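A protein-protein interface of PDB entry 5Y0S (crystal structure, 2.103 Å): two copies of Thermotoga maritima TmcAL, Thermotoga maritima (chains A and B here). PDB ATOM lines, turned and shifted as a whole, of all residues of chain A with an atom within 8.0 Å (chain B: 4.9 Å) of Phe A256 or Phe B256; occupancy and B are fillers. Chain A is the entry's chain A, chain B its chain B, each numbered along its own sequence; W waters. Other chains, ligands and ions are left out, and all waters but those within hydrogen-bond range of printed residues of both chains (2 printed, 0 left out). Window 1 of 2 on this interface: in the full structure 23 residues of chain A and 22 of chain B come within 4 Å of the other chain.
CB of Ser B259 touches CE2 of Phe A256, at 3.6 Å.
CZ of Phe A256 touches CD1 of Leu B263, 3.8 Å away.
Phe B256 touches Ser A259.
N of Phe A260 touches CE1 of Phe B256 (3.6 Å).
CE2 of Phe B260 touches CE2 of Phe A260, at 3.8 Å.
CD1 of Phe B397 touches CD2 of Leu A263 (3.8 Å).
Phe A319 touches Leu B263 (CD1 to CD2, 3.9 Å).
Leu B263 touches Phe A397.
Leu B258 touches Met A400.
Met A400 touches Ser B259.
The backbone carbonyl oxygen (O) of Asp A255 is in hydrogen-bond range of the side-chain hydroxyl (OG) of Ser A259, at 2.8 Å.
The backbone carbonyl oxygen of Asp B255 lies within hydrogen-bond range of the side-chain hydroxyl of Ser B259, at 2.7 Å.
Phe A256 touches Ser B259, and with the chains exchanged Ser A259 touches Phe B256.
Phe B260 touches its own counterpart, Phe A260.
Leu A263 touches Val B318, and with the chains exchanged Val A318 touches Leu B263.
Leu A263 touches Phe B397, and with the chains exchanged Phe A397 touches Leu B263.
Positions printed for both chains: 253, 254, 255, 256, 257, 258, 259, 260, 263, 318, 397 and 401.
Of the 15 pairs that touch across the chains among the printed residues, 12 have their exchanged pair printed and touching as well.
Printed residues of chain A that touch a printed residue of chain B: Phe A256, Ser A259, Phe A260, Leu A263, Val A318, Phe A319, Phe A397 and Met A400.
Hydrophobic or aromatic side chains of chain A that line the printed part of chain B: Phe A256, Phe A260, Leu A263, Phe A319, Phe A397 and Met A400.
Of the 12 printed residues of chain B, 7 touch a printed residue of chain A.
Printed residues of chain B that touch a printed residue of chain A: Phe B256, Leu B258, Ser B259, Phe B260, Leu B263, Val B318 and Phe B397.
Among the printed residues, 15 pairs touch across the chains.
Among the printed residues, no Asp or Glu carboxylate lies within 4 Å of a Lys or Arg side-chain nitrogen of the other chain.
Water W2 bridges the backbone carbonyl oxygen of Met A400 (2.7 Å) and the side-chain carboxylate of Asp B255 (3.0 Å).
Water W1 bridges O of Val B318 (2.8 Å) and NZ of Lys A264 (3.4 Å).
Phe A256 touches four residues of chain B.
Of the printed residues of chain B, Phe A260 touches Phe B256 (3.6 Å) and Phe B260 (3.8 Å).
Of the printed residues of chain B, Met A400 touches Leu B258 (3.8 Å) and Ser B259 (3.4 Å).
Phe B256 touches just these residues of chain A: Phe A256 (3.3 Å), Ser A259 (3.5 Å), Phe A260 (3.6 Å) and Leu A263 (3.7 Å).
The nearest residue of chain A that does not touch Phe B256 is Asp A255 (5.0 Å).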
ATOM      1  N   LEU A 250     -21.142  23.204  12.292  1.00  0.00           N
ATOM      2  CA  LEU A 250     -19.794  22.676  12.074  1.00  0.00           C
ATOM      3  C   LEU A 250     -18.823  23.164  13.154  1.00  0.00           C
ATOM      4  O   LEU A 250     -17.943  22.431  13.580  1.00  0.00           O
ATOM      5  CB  LEU A 250     -19.283  23.064  10.682  1.00  0.00           C
ATOM      6  CG  LEU A 250     -17.876  22.594  10.303  1.00  0.00           C
ATOM      7  CD1 LEU A 250     -17.719  21.084  10.387  1.00  0.00           C
ATOM      8  CD2 LEU A 250     -17.538  23.078   8.911  1.00  0.00           C
ATOM      9  N   GLU A 251     -19.005  24.398  13.616  1.00  0.00           N
ATOM     10  CA  GLU A 251     -18.076  24.968  14.567  1.00  0.00           C
ATOM     11  C   GLU A 251     -18.161  24.231  15.910  1.00  0.00           C
ATOM     12  O   GLU A 251     -17.186  24.215  16.662  1.00  0.00           O
ATOM     13  CB  GLU A 251     -18.313  26.480  14.740  1.00  0.00           C
ATOM     14  CG  GLU A 251     -19.728  26.872  15.148  1.00  0.00           C
ATOM     15  CD  GLU A 251     -20.614  27.289  13.962  1.00  0.00           C
ATOM     16  OE1 GLU A 251     -20.441  26.754  12.840  1.00  0.00           O
ATOM     17  OE2 GLU A 251     -21.487  28.163  14.168  1.00  0.00           O
ATOM     18  N   ASN A 252     -19.299  23.591  16.192  1.00  0.00           N
ATOM     19  CA  ASN A 252     -19.402  22.759  17.385  1.00  0.00           C
ATOM     20  C   ASN A 252     -18.426  21.582  17.329  1.00  0.00           C
ATOM     21  O   ASN A 252     -17.949  21.113  18.357  1.00  0.00           O
ATOM     22  CB  ASN A 252     -20.830  22.220  17.578  1.00  0.00           C
ATOM     23  CG  ASN A 252     -21.878  23.322  17.691  1.00  0.00           C
ATOM     24  OD1 ASN A 252     -23.013  23.164  17.220  1.00  0.00           O
ATOM     25  ND2 ASN A 252     -21.511  24.435  18.314  1.00  0.00           N
ATOM     26  N   MET A 253     -18.152  21.089  16.126  1.00  0.00           N
ATOM     27  CA  MET A 253     -17.210  19.982  15.940  1.00  0.00           C
ATOM     28  C   MET A 253     -15.779  20.444  15.710  1.00  0.00           C
ATOM     29  O   MET A 253     -14.875  19.622  15.527  1.00  0.00           O
ATOM     30  CB  MET A 253     -17.637  19.130  14.745  1.00  0.00           C
ATOM     31  CG  MET A 253     -18.946  18.411  14.930  1.00  0.00           C
ATOM     32  SD  MET A 253     -19.611  17.822  13.353  1.00  0.00           S
ATOM     33  CE  MET A 253     -21.107  17.040  13.949  1.00  0.00           C
ATOM     34  N   GLY A 254     -15.580  21.757  15.668  1.00  0.00           N
ATOM     35  CA  GLY A 254     -14.314  22.308  15.223  1.00  0.00           C
ATOM     36  C   GLY A 254     -13.122  21.929  16.087  1.00  0.00           C
ATOM     37  O   GLY A 254     -12.066  21.552  15.565  1.00  0.00           O
ATOM     38  N   ASP A 255     -13.276  22.016  17.406  1.00  0.00           N
ATOM     39  CA  ASP A 255     -12.162  21.673  18.304  1.00  0.00           C
ATOM     40  C   ASP A 255     -11.832  20.188  18.201  1.00  0.00           C
ATOM     41  O   ASP A 255     -10.657  19.804  18.287  1.00  0.00           O
ATOM     42  CB  ASP A 255     -12.470  22.034  19.756  1.00  0.00           C
ATOM     43  CG  ASP A 255     -12.232  23.507  20.069  1.00  0.00           C
ATOM     44  OD1 ASP A 255     -11.791  24.258  19.174  1.00  0.00           O
ATOM     45  OD2 ASP A 255     -12.493  23.917  21.222  1.00  0.00           O
ATOM     46  N   PHE A 256     -12.851  19.354  18.012  1.00  0.00           N
ATOM     47  CA  PHE A 256     -12.596  17.924  17.874  1.00  0.00           C
ATOM     48  C   PHE A 256     -11.715  17.656  16.669  1.00  0.00           C
ATOM     49  O   PHE A 256     -10.693  16.973  16.780  1.00  0.00           O
ATOM     50  CB  PHE A 256     -13.873  17.078  17.730  1.00  0.00           C
ATOM     51  CG  PHE A 256     -13.566  15.602  17.715  1.00  0.00           C
ATOM     52  CD1 PHE A 256     -13.233  14.955  16.532  1.00  0.00           C
ATOM     53  CD2 PHE A 256     -13.513  14.886  18.900  1.00  0.00           C
ATOM     54  CE1 PHE A 256     -12.887  13.612  16.535  1.00  0.00           C
ATOM     55  CE2 PHE A 256     -13.173  13.546  18.911  1.00  0.00           C
ATOM     56  CZ  PHE A 256     -12.859  12.908  17.728  1.00  0.00           C
ATOM     57  N   LEU A 257     -12.153  18.164  15.518  1.00  0.00           N
ATOM     58  CA  LEU A 257     -11.462  17.967  14.248  1.00  0.00           C
ATOM     59  C   LEU A 257     -10.016  18.414  14.313  1.00  0.00           C
ATOM     60  O   LEU A 257      -9.118  17.720  13.841  1.00  0.00           O
ATOM     61  CB  LEU A 257     -12.185  18.725  13.127  1.00  0.00           C
ATOM     62  CG  LEU A 257     -13.577  18.185  12.798  1.00  0.00           C
ATOM     63  CD1 LEU A 257     -14.257  19.008  11.705  1.00  0.00           C
ATOM     64  CD2 LEU A 257     -13.489  16.736  12.392  1.00  0.00           C
ATOM     65  N   LEU A 258      -9.794  19.579  14.910  1.00  0.00           N
ATOM     66  CA  LEU A 258      -8.469  20.148  14.953  1.00  0.00           C
ATOM     67  C   LEU A 258      -7.575  19.340  15.916  1.00  0.00           C
ATOM     68  O   LEU A 258      -6.429  19.048  15.597  1.00  0.00           O
ATOM     69  CB  LEU A 258      -8.540  21.624  15.344  1.00  0.00           C
ATOM     70  CG  LEU A 258      -7.207  22.364  15.462  1.00  0.00           C
ATOM     71  CD1 LEU A 258      -6.426  22.224  14.180  1.00  0.00           C
ATOM     72  CD2 LEU A 258      -7.418  23.836  15.804  1.00  0.00           C
ATOM     73  N   SER A 259      -8.112  18.957  17.070  1.00  0.00           N
ATOM     74  CA  SER A 259      -7.381  18.113  18.022  1.00  0.00           C
ATOM     75  C   SER A 259      -7.053  16.734  17.421  1.00  0.00           C
ATOM     76  O   SER A 259      -5.965  16.193  17.619  1.00  0.00           O
ATOM     77  CB  SER A 259      -8.190  17.941  19.320  1.00  0.00           C
ATOM     78  OG  SER A 259      -8.429  19.196  19.951  1.00  0.00           O
ATOM     79  N   PHE A 260      -8.001  16.183  16.675  1.00  0.00           N
ATOM     80  CA  PHE A 260      -7.827  14.918  15.973  1.00  0.00           C
ATOM     81  C   PHE A 260      -6.687  14.986  14.937  1.00  0.00           C
ATOM     82  O   PHE A 260      -5.855  14.079  14.847  1.00  0.00           O
ATOM     83  CB  PHE A 260      -9.156  14.526  15.308  1.00  0.00           C
ATOM     84  CG  PHE A 260      -9.128  13.189  14.614  1.00  0.00           C
ATOM     85  CD1 PHE A 260      -8.723  13.087  13.288  1.00  0.00           C
ATOM     86  CD2 PHE A 260      -9.542  12.040  15.274  1.00  0.00           C
ATOM     87  CE1 PHE A 260      -8.706  11.861  12.641  1.00  0.00           C
ATOM     88  CE2 PHE A 260      -9.518  10.815  14.635  1.00  0.00           C
ATOM     89  CZ  PHE A 260      -9.104  10.727  13.315  1.00  0.00           C
ATOM     90  N   PHE A 261      -6.622  16.072  14.175  1.00  0.00           N
ATOM     91  CA  PHE A 261      -5.564  16.200  13.171  1.00  0.00           C
ATOM     92  C   PHE A 261      -4.191  16.341  13.832  1.00  0.00           C
ATOM     93  O   PHE A 261      -3.184  15.927  13.264  1.00  0.00           O
ATOM     94  CB  PHE A 261      -5.833  17.383  12.232  1.00  0.00           C
ATOM     95  CG  PHE A 261      -7.143  17.298  11.508  1.00  0.00           C
ATOM     96  CD1 PHE A 261      -7.740  16.072  11.256  1.00  0.00           C
ATOM     97  CD2 PHE A 261      -7.791  18.452  11.087  1.00  0.00           C
ATOM     98  CE1 PHE A 261      -8.964  16.000  10.602  1.00  0.00           C
ATOM     99  CE2 PHE A 261      -9.011  18.387  10.434  1.00  0.00           C
ATOM    100  CZ  PHE A 261      -9.601  17.165  10.190  1.00  0.00           C
ATOM    101  N   ARG A 262      -4.145  16.887  15.045  1.00  0.00           N
ATOM    102  CA  ARG A 262      -2.883  16.939  15.790  1.00  0.00           C
ATOM    103  C   ARG A 262      -2.387  15.580  16.246  1.00  0.00           C
ATOM    104  O   ARG A 262      -1.253  15.449  16.695  1.00  0.00           O
ATOM    105  CB  ARG A 262      -3.007  17.829  17.018  1.00  0.00           C
ATOM    106  CG  ARG A 262      -3.156  19.266  16.682  1.00  0.00           C
ATOM    107  CD  ARG A 262      -2.923  20.118  17.886  1.00  0.00           C
ATOM    108  NE  ARG A 262      -3.033  21.512  17.499  1.00  0.00           N
ATOM    109  CZ  ARG A 262      -2.781  22.527  18.305  1.00  0.00           C
ATOM    110  NH1 ARG A 262      -2.393  22.298  19.552  1.00  0.00           N
ATOM    111  NH2 ARG A 262      -2.905  23.767  17.851  1.00  0.00           N
ATOM    112  N   LEU A 263      -3.238  14.569  16.165  1.00  0.00           N
ATOM    113  CA  LEU A 263      -2.820  13.228  16.536  1.00  0.00           C
ATOM    114  C   LEU A 263      -2.206  12.471  15.354  1.00  0.00           C
ATOM    115  O   LEU A 263      -1.627  11.404  15.525  1.00  0.00           O
ATOM    116  CB  LEU A 263      -4.012  12.446  17.094  1.00  0.00           C
ATOM    117  CG  LEU A 263      -4.666  13.072  18.335  1.00  0.00           C
ATOM    118  CD1 LEU A 263      -5.959  12.325  18.763  1.00  0.00           C
ATOM    119  CD2 LEU A 263      -3.646  13.117  19.473  1.00  0.00           C
ATOM    120  N   LYS A 264      -2.344  13.021  14.155  1.00  0.00           N
ATOM    121  CA  LYS A 264      -2.003  12.275  12.951  1.00  0.00           C
ATOM    122  C   LYS A 264      -0.776  12.836  12.245  1.00  0.00           C
ATOM    123  O   LYS A 264      -0.537  14.041  12.280  1.00  0.00           O
ATOM    124  CB  LYS A 264      -3.193  12.275  11.992  1.00  0.00           C
ATOM    125  CG  LYS A 264      -4.475  11.745  12.611  1.00  0.00           C
ATOM    126  CD  LYS A 264      -4.303  10.317  13.097  1.00  0.00           C
ATOM    127  CE  LYS A 264      -5.606   9.801  13.717  1.00  0.00           C
ATOM    128  NZ  LYS A 264      -5.587   8.325  13.876  1.00  0.00           N
ATOM    129  N   TYR A 293     -10.713  25.746  14.414  1.00  0.00           N
ATOM    130  CA  TYR A 293     -10.983  25.087  13.147  1.00  0.00           C
ATOM    131  C   TYR A 293     -11.192  26.110  12.037  1.00  0.00           C
ATOM    132  O   TYR A 293     -10.815  25.877  10.888  1.00  0.00           O
ATOM    133  CB  TYR A 293     -12.193  24.175  13.289  1.00  0.00           C
ATOM    134  CG  TYR A 293     -12.491  23.331  12.076  1.00  0.00           C
ATOM    135  CD1 TYR A 293     -11.502  22.559  11.475  1.00  0.00           C
ATOM    136  CD2 TYR A 293     -13.768  23.298  11.533  1.00  0.00           C
ATOM    137  CE1 TYR A 293     -11.783  21.783  10.354  1.00  0.00           C
ATOM    138  CE2 TYR A 293     -14.058  22.520  10.434  1.00  0.00           C
ATOM    139  CZ  TYR A 293     -13.064  21.768   9.847  1.00  0.00           C
ATOM    140  OH  TYR A 293     -13.369  21.002   8.748  1.00  0.00           O
ATOM    141  N   ALA A 314     -11.671  17.052   5.778  1.00  0.00           N
ATOM    142  CA  ALA A 314     -11.662  16.920   7.234  1.00  0.00           C
ATOM    143  C   ALA A 314     -12.587  15.797   7.695  1.00  0.00           C
ATOM    144  O   ALA A 314     -12.267  15.072   8.651  1.00  0.00           O
ATOM    145  CB  ALA A 314     -12.064  18.236   7.899  1.00  0.00           C
ATOM    146  N   VAL A 318     -11.476  12.335   9.704  1.00  0.00           N
ATOM    147  CA  VAL A 318     -11.977  11.979  11.015  1.00  0.00           C
ATOM    148  C   VAL A 318     -12.692  10.619  10.951  1.00  0.00           C
ATOM    149  O   VAL A 318     -12.670   9.874  11.915  1.00  0.00           O
ATOM    150  CB  VAL A 318     -12.911  13.097  11.582  1.00  0.00           C
ATOM    151  CG1 VAL A 318     -14.339  13.002  11.003  1.00  0.00           C
ATOM    152  CG2 VAL A 318     -12.937  13.055  13.087  1.00  0.00           C
ATOM    153  N   PHE A 319     -13.296  10.283   9.808  1.00  0.00           N
ATOM    154  CA  PHE A 319     -14.003   9.010   9.670  1.00  0.00           C
ATOM    155  C   PHE A 319     -13.125   7.935   9.019  1.00  0.00           C
ATOM    156  O   PHE A 319     -13.583   6.821   8.759  1.00  0.00           O
ATOM    157  CB  PHE A 319     -15.290   9.196   8.857  1.00  0.00           C
ATOM    158  CG  PHE A 319     -16.325  10.042   9.548  1.00  0.00           C
ATOM    159  CD1 PHE A 319     -16.589   9.874  10.901  1.00  0.00           C
ATOM    160  CD2 PHE A 319     -17.034  11.009   8.844  1.00  0.00           C
ATOM    161  CE1 PHE A 319     -17.553  10.650  11.546  1.00  0.00           C
ATOM    162  CE2 PHE A 319     -17.989  11.790   9.480  1.00  0.00           C
ATOM    163  CZ  PHE A 319     -18.247  11.611  10.830  1.00  0.00           C
ATOM    164  N   PHE A 397     -21.080   9.687  15.973  1.00  0.00           N
ATOM    165  CA  PHE A 397     -20.239  10.868  16.160  1.00  0.00           C
ATOM    166  C   PHE A 397     -21.104  12.135  16.227  1.00  0.00           C
ATOM    167  O   PHE A 397     -20.982  12.936  17.153  1.00  0.00           O
ATOM    168  CB  PHE A 397     -19.220  10.953  15.026  1.00  0.00           C
ATOM    169  CG  PHE A 397     -18.272  12.109  15.137  1.00  0.00           C
ATOM    170  CD1 PHE A 397     -17.259  12.108  16.088  1.00  0.00           C
ATOM    171  CD2 PHE A 397     -18.364  13.181  14.261  1.00  0.00           C
ATOM    172  CE1 PHE A 397     -16.357  13.184  16.173  1.00  0.00           C
ATOM    173  CE2 PHE A 397     -17.472  14.247  14.338  1.00  0.00           C
ATOM    174  CZ  PHE A 397     -16.465  14.246  15.296  1.00  0.00           C
ATOM    175  N   MET A 400     -22.883  13.145  19.570  1.00  0.00           N
ATOM    176  CA  MET A 400     -22.106  13.711  20.674  1.00  0.00           C
ATOM    177  C   MET A 400     -22.212  15.228  20.657  1.00  0.00           C
ATOM    178  O   MET A 400     -21.907  15.883  21.646  1.00  0.00           O
ATOM    179  CB  MET A 400     -20.625  13.283  20.609  1.00  0.00           C
ATOM    180  CG  MET A 400     -20.332  11.905  21.241  1.00  0.00           C
ATOM    181  SD  MET A 400     -20.927  11.744  22.932  1.00  0.00           S
ATOM    182  CE  MET A 400     -19.994  13.052  23.752  1.00  0.00           C
ATOM    183  N   PHE A 401     -22.634  15.785  19.522  1.00  0.00           N
ATOM    184  CA  PHE A 401     -22.707  17.236  19.373  1.00  0.00           C
ATOM    185  C   PHE A 401     -24.120  17.813  19.521  1.00  0.00           C
ATOM    186  O   PHE A 401     -24.322  19.018  19.373  1.00  0.00           O
ATOM    187  CB  PHE A 401     -22.041  17.617  18.047  1.00  0.00           C
ATOM    188  CG  PHE A 401     -20.590  17.234  18.019  1.00  0.00           C
ATOM    189  CD1 PHE A 401     -19.629  18.073  18.569  1.00  0.00           C
ATOM    190  CD2 PHE A 401     -20.196  15.992  17.547  1.00  0.00           C
ATOM    191  CE1 PHE A 401     -18.279  17.708  18.587  1.00  0.00           C
ATOM    192  CE2 PHE A 401     -18.857  15.608  17.569  1.00  0.00           C
ATOM    193  CZ  PHE A 401     -17.892  16.473  18.089  1.00  0.00           C
ATOM    194  N   MET B 253     -11.109  17.232  28.623  1.00  0.00           N
ATOM    195  CA  MET B 253     -10.837  16.326  27.513  1.00  0.00           C
ATOM    196  C   MET B 253     -11.903  15.237  27.325  1.00  0.00           C
ATOM    197  O   MET B 253     -11.809  14.417  26.409  1.00  0.00           O
ATOM    198  CB  MET B 253      -9.469  15.665  27.723  1.00  0.00           C
ATOM    199  CG  MET B 253      -8.346  16.667  27.806  1.00  0.00           C
ATOM    200  SD  MET B 253      -6.783  15.953  28.373  1.00  0.00           S
ATOM    201  CE  MET B 253      -5.683  17.283  27.879  1.00  0.00           C
ATOM    202  N   GLY B 254     -12.907  15.220  28.195  1.00  0.00           N
ATOM    203  CA  GLY B 254     -13.824  14.098  28.244  1.00  0.00           C
ATOM    204  C   GLY B 254     -14.639  13.867  26.979  1.00  0.00           C
ATOM    205  O   GLY B 254     -14.764  12.737  26.507  1.00  0.00           O
ATOM    206  N   ASP B 255     -15.195  14.932  26.420  1.00  0.00           N
ATOM    207  CA  ASP B 255     -15.979  14.783  25.194  1.00  0.00           C
ATOM    208  C   ASP B 255     -15.109  14.350  24.024  1.00  0.00           C
ATOM    209  O   ASP B 255     -15.577  13.612  23.163  1.00  0.00           O
ATOM    210  CB  ASP B 255     -16.703  16.083  24.840  1.00  0.00           C
ATOM    211  CG  ASP B 255     -17.984  16.257  25.607  1.00  0.00           C
ATOM    212  OD1 ASP B 255     -18.250  15.425  26.512  1.00  0.00           O
ATOM    213  OD2 ASP B 255     -18.724  17.223  25.300  1.00  0.00           O
ATOM    214  N   PHE B 256     -13.853  14.805  23.975  1.00  0.00           N
ATOM    215  CA  PHE B 256     -12.969  14.342  22.905  1.00  0.00           C
ATOM    216  C   PHE B 256     -12.742  12.831  22.995  1.00  0.00           C
ATOM    217  O   PHE B 256     -12.885  12.099  22.011  1.00  0.00           O
ATOM    218  CB  PHE B 256     -11.592  15.037  22.919  1.00  0.00           C
ATOM    219  CG  PHE B 256     -10.736  14.635  21.744  1.00  0.00           C
ATOM    220  CD1 PHE B 256     -10.729  15.397  20.587  1.00  0.00           C
ATOM    221  CD2 PHE B 256     -10.029  13.434  21.752  1.00  0.00           C
ATOM    222  CE1 PHE B 256      -9.993  14.998  19.480  1.00  0.00           C
ATOM    223  CE2 PHE B 256      -9.310  13.024  20.649  1.00  0.00           C
ATOM    224  CZ  PHE B 256      -9.289  13.822  19.508  1.00  0.00           C
ATOM    225  N   LEU B 257     -12.339  12.384  24.179  1.00  0.00           N
ATOM    226  CA  LEU B 257     -12.055  10.976  24.418  1.00  0.00           C
ATOM    227  C   LEU B 257     -13.264  10.105  24.082  1.00  0.00           C
ATOM    228  O   LEU B 257     -13.133   9.065  23.443  1.00  0.00           O
ATOM    229  CB  LEU B 257     -11.640  10.764  25.881  1.00  0.00           C
ATOM    230  CG  LEU B 257     -10.329  11.398  26.322  1.00  0.00           C
ATOM    231  CD1 LEU B 257     -10.121  11.183  27.821  1.00  0.00           C
ATOM    232  CD2 LEU B 257      -9.188  10.801  25.536  1.00  0.00           C
ATOM    233  N   LEU B 258     -14.442  10.540  24.519  1.00  0.00           N
ATOM    234  CA  LEU B 258     -15.654   9.752  24.327  1.00  0.00           C
ATOM    235  C   LEU B 258     -16.030   9.704  22.845  1.00  0.00           C
ATOM    236  O   LEU B 258     -16.352   8.642  22.307  1.00  0.00           O
ATOM    237  CB  LEU B 258     -16.814  10.320  25.153  1.00  0.00           C
ATOM    238  CG  LEU B 258     -18.131   9.535  25.063  1.00  0.00           C
ATOM    239  CD1 LEU B 258     -17.902   8.044  25.321  1.00  0.00           C
ATOM    240  CD2 LEU B 258     -19.176  10.079  26.031  1.00  0.00           C
ATOM    241  N   SER B 259     -15.980  10.852  22.185  1.00  0.00           N
ATOM    242  CA  SER B 259     -16.294  10.905  20.758  1.00  0.00           C
ATOM    243  C   SER B 259     -15.318  10.049  19.942  1.00  0.00           C
ATOM    244  O   SER B 259     -15.716   9.361  18.997  1.00  0.00           O
ATOM    245  CB  SER B 259     -16.267  12.350  20.253  1.00  0.00           C
ATOM    246  OG  SER B 259     -17.162  13.177  20.976  1.00  0.00           O
ATOM    247  N   PHE B 260     -14.047  10.095  20.328  1.00  0.00           N
ATOM    248  CA  PHE B 260     -12.984   9.363  19.638  1.00  0.00           C
ATOM    249  C   PHE B 260     -13.264   7.856  19.704  1.00  0.00           C
ATOM    250  O   PHE B 260     -13.119   7.135  18.719  1.00  0.00           O
ATOM    251  CB  PHE B 260     -11.625   9.719  20.271  1.00  0.00           C
ATOM    252  CG  PHE B 260     -10.426   9.084  19.602  1.00  0.00           C
ATOM    253  CD1 PHE B 260      -9.948   7.849  20.028  1.00  0.00           C
ATOM    254  CD2 PHE B 260      -9.740   9.752  18.590  1.00  0.00           C
ATOM    255  CE1 PHE B 260      -8.829   7.277  19.440  1.00  0.00           C
ATOM    256  CE2 PHE B 260      -8.613   9.186  17.996  1.00  0.00           C
ATOM    257  CZ  PHE B 260      -8.157   7.944  18.424  1.00  0.00           C
ATOM    258  N   LEU B 263     -15.491   6.357  17.100  1.00  0.00           N
ATOM    259  CA  LEU B 263     -14.954   6.237  15.754  1.00  0.00           C
ATOM    260  C   LEU B 263     -14.238   4.893  15.564  1.00  0.00           C
ATOM    261  O   LEU B 263     -13.850   4.533  14.450  1.00  0.00           O
ATOM    262  CB  LEU B 263     -13.988   7.386  15.479  1.00  0.00           C
ATOM    263  CG  LEU B 263     -14.529   8.808  15.657  1.00  0.00           C
ATOM    264  CD1 LEU B 263     -13.386   9.829  15.607  1.00  0.00           C
ATOM    265  CD2 LEU B 263     -15.582   9.118  14.590  1.00  0.00           C
ATOM    266  N   VAL B 318      -6.200   7.155  22.513  1.00  0.00           N
ATOM    267  CA  VAL B 318      -6.185   8.348  21.653  1.00  0.00           C
ATOM    268  C   VAL B 318      -4.817   8.609  21.081  1.00  0.00           C
ATOM    269  O   VAL B 318      -4.716   9.151  20.000  1.00  0.00           O
ATOM    270  CB  VAL B 318      -6.637   9.658  22.350  1.00  0.00           C
ATOM    271  CG1 VAL B 318      -8.133   9.680  22.503  1.00  0.00           C
ATOM    272  CG2 VAL B 318      -5.891   9.886  23.662  1.00  0.00           C
ATOM    273  N   PHE B 397      -1.587  17.802  21.718  1.00  0.00           N
ATOM    274  CA  PHE B 397      -2.964  17.484  22.083  1.00  0.00           C
ATOM    275  C   PHE B 397      -3.359  18.267  23.332  1.00  0.00           C
ATOM    276  O   PHE B 397      -4.398  18.923  23.363  1.00  0.00           O
ATOM    277  CB  PHE B 397      -3.134  15.976  22.313  1.00  0.00           C
ATOM    278  CG  PHE B 397      -4.538  15.568  22.683  1.00  0.00           C
ATOM    279  CD1 PHE B 397      -5.545  15.528  21.723  1.00  0.00           C
ATOM    280  CD2 PHE B 397      -4.847  15.201  23.988  1.00  0.00           C
ATOM    281  CE1 PHE B 397      -6.849  15.130  22.063  1.00  0.00           C
ATOM    282  CE2 PHE B 397      -6.137  14.801  24.329  1.00  0.00           C
ATOM    283  CZ  PHE B 397      -7.140  14.773  23.361  1.00  0.00           C
ATOM    284  N   PHE B 401      -6.427  22.155  24.976  1.00  0.00           N
ATOM    285  CA  PHE B 401      -7.299  22.310  26.139  1.00  0.00           C
ATOM    286  C   PHE B 401      -6.898  23.466  27.068  1.00  0.00           C
ATOM    287  O   PHE B 401      -7.468  23.612  28.145  1.00  0.00           O
ATOM    288  CB  PHE B 401      -7.384  20.965  26.871  1.00  0.00           C
ATOM    289  CG  PHE B 401      -7.900  19.881  25.987  1.00  0.00           C
ATOM    290  CD1 PHE B 401      -9.276  19.687  25.834  1.00  0.00           C
ATOM    291  CD2 PHE B 401      -7.028  19.132  25.207  1.00  0.00           C
ATOM    292  CE1 PHE B 401      -9.770  18.718  24.973  1.00  0.00           C
ATOM    293  CE2 PHE B 401      -7.511  18.166  24.330  1.00  0.00           C
ATOM    294  CZ  PHE B 401      -8.887  17.953  24.216  1.00  0.00           C
HETATM  295  O   HOH W   1      -4.983   8.844  17.195  1.00  0.00           O
HETATM  296  O   HOH W   2     -19.579  17.104  22.388  1.00  0.00           O
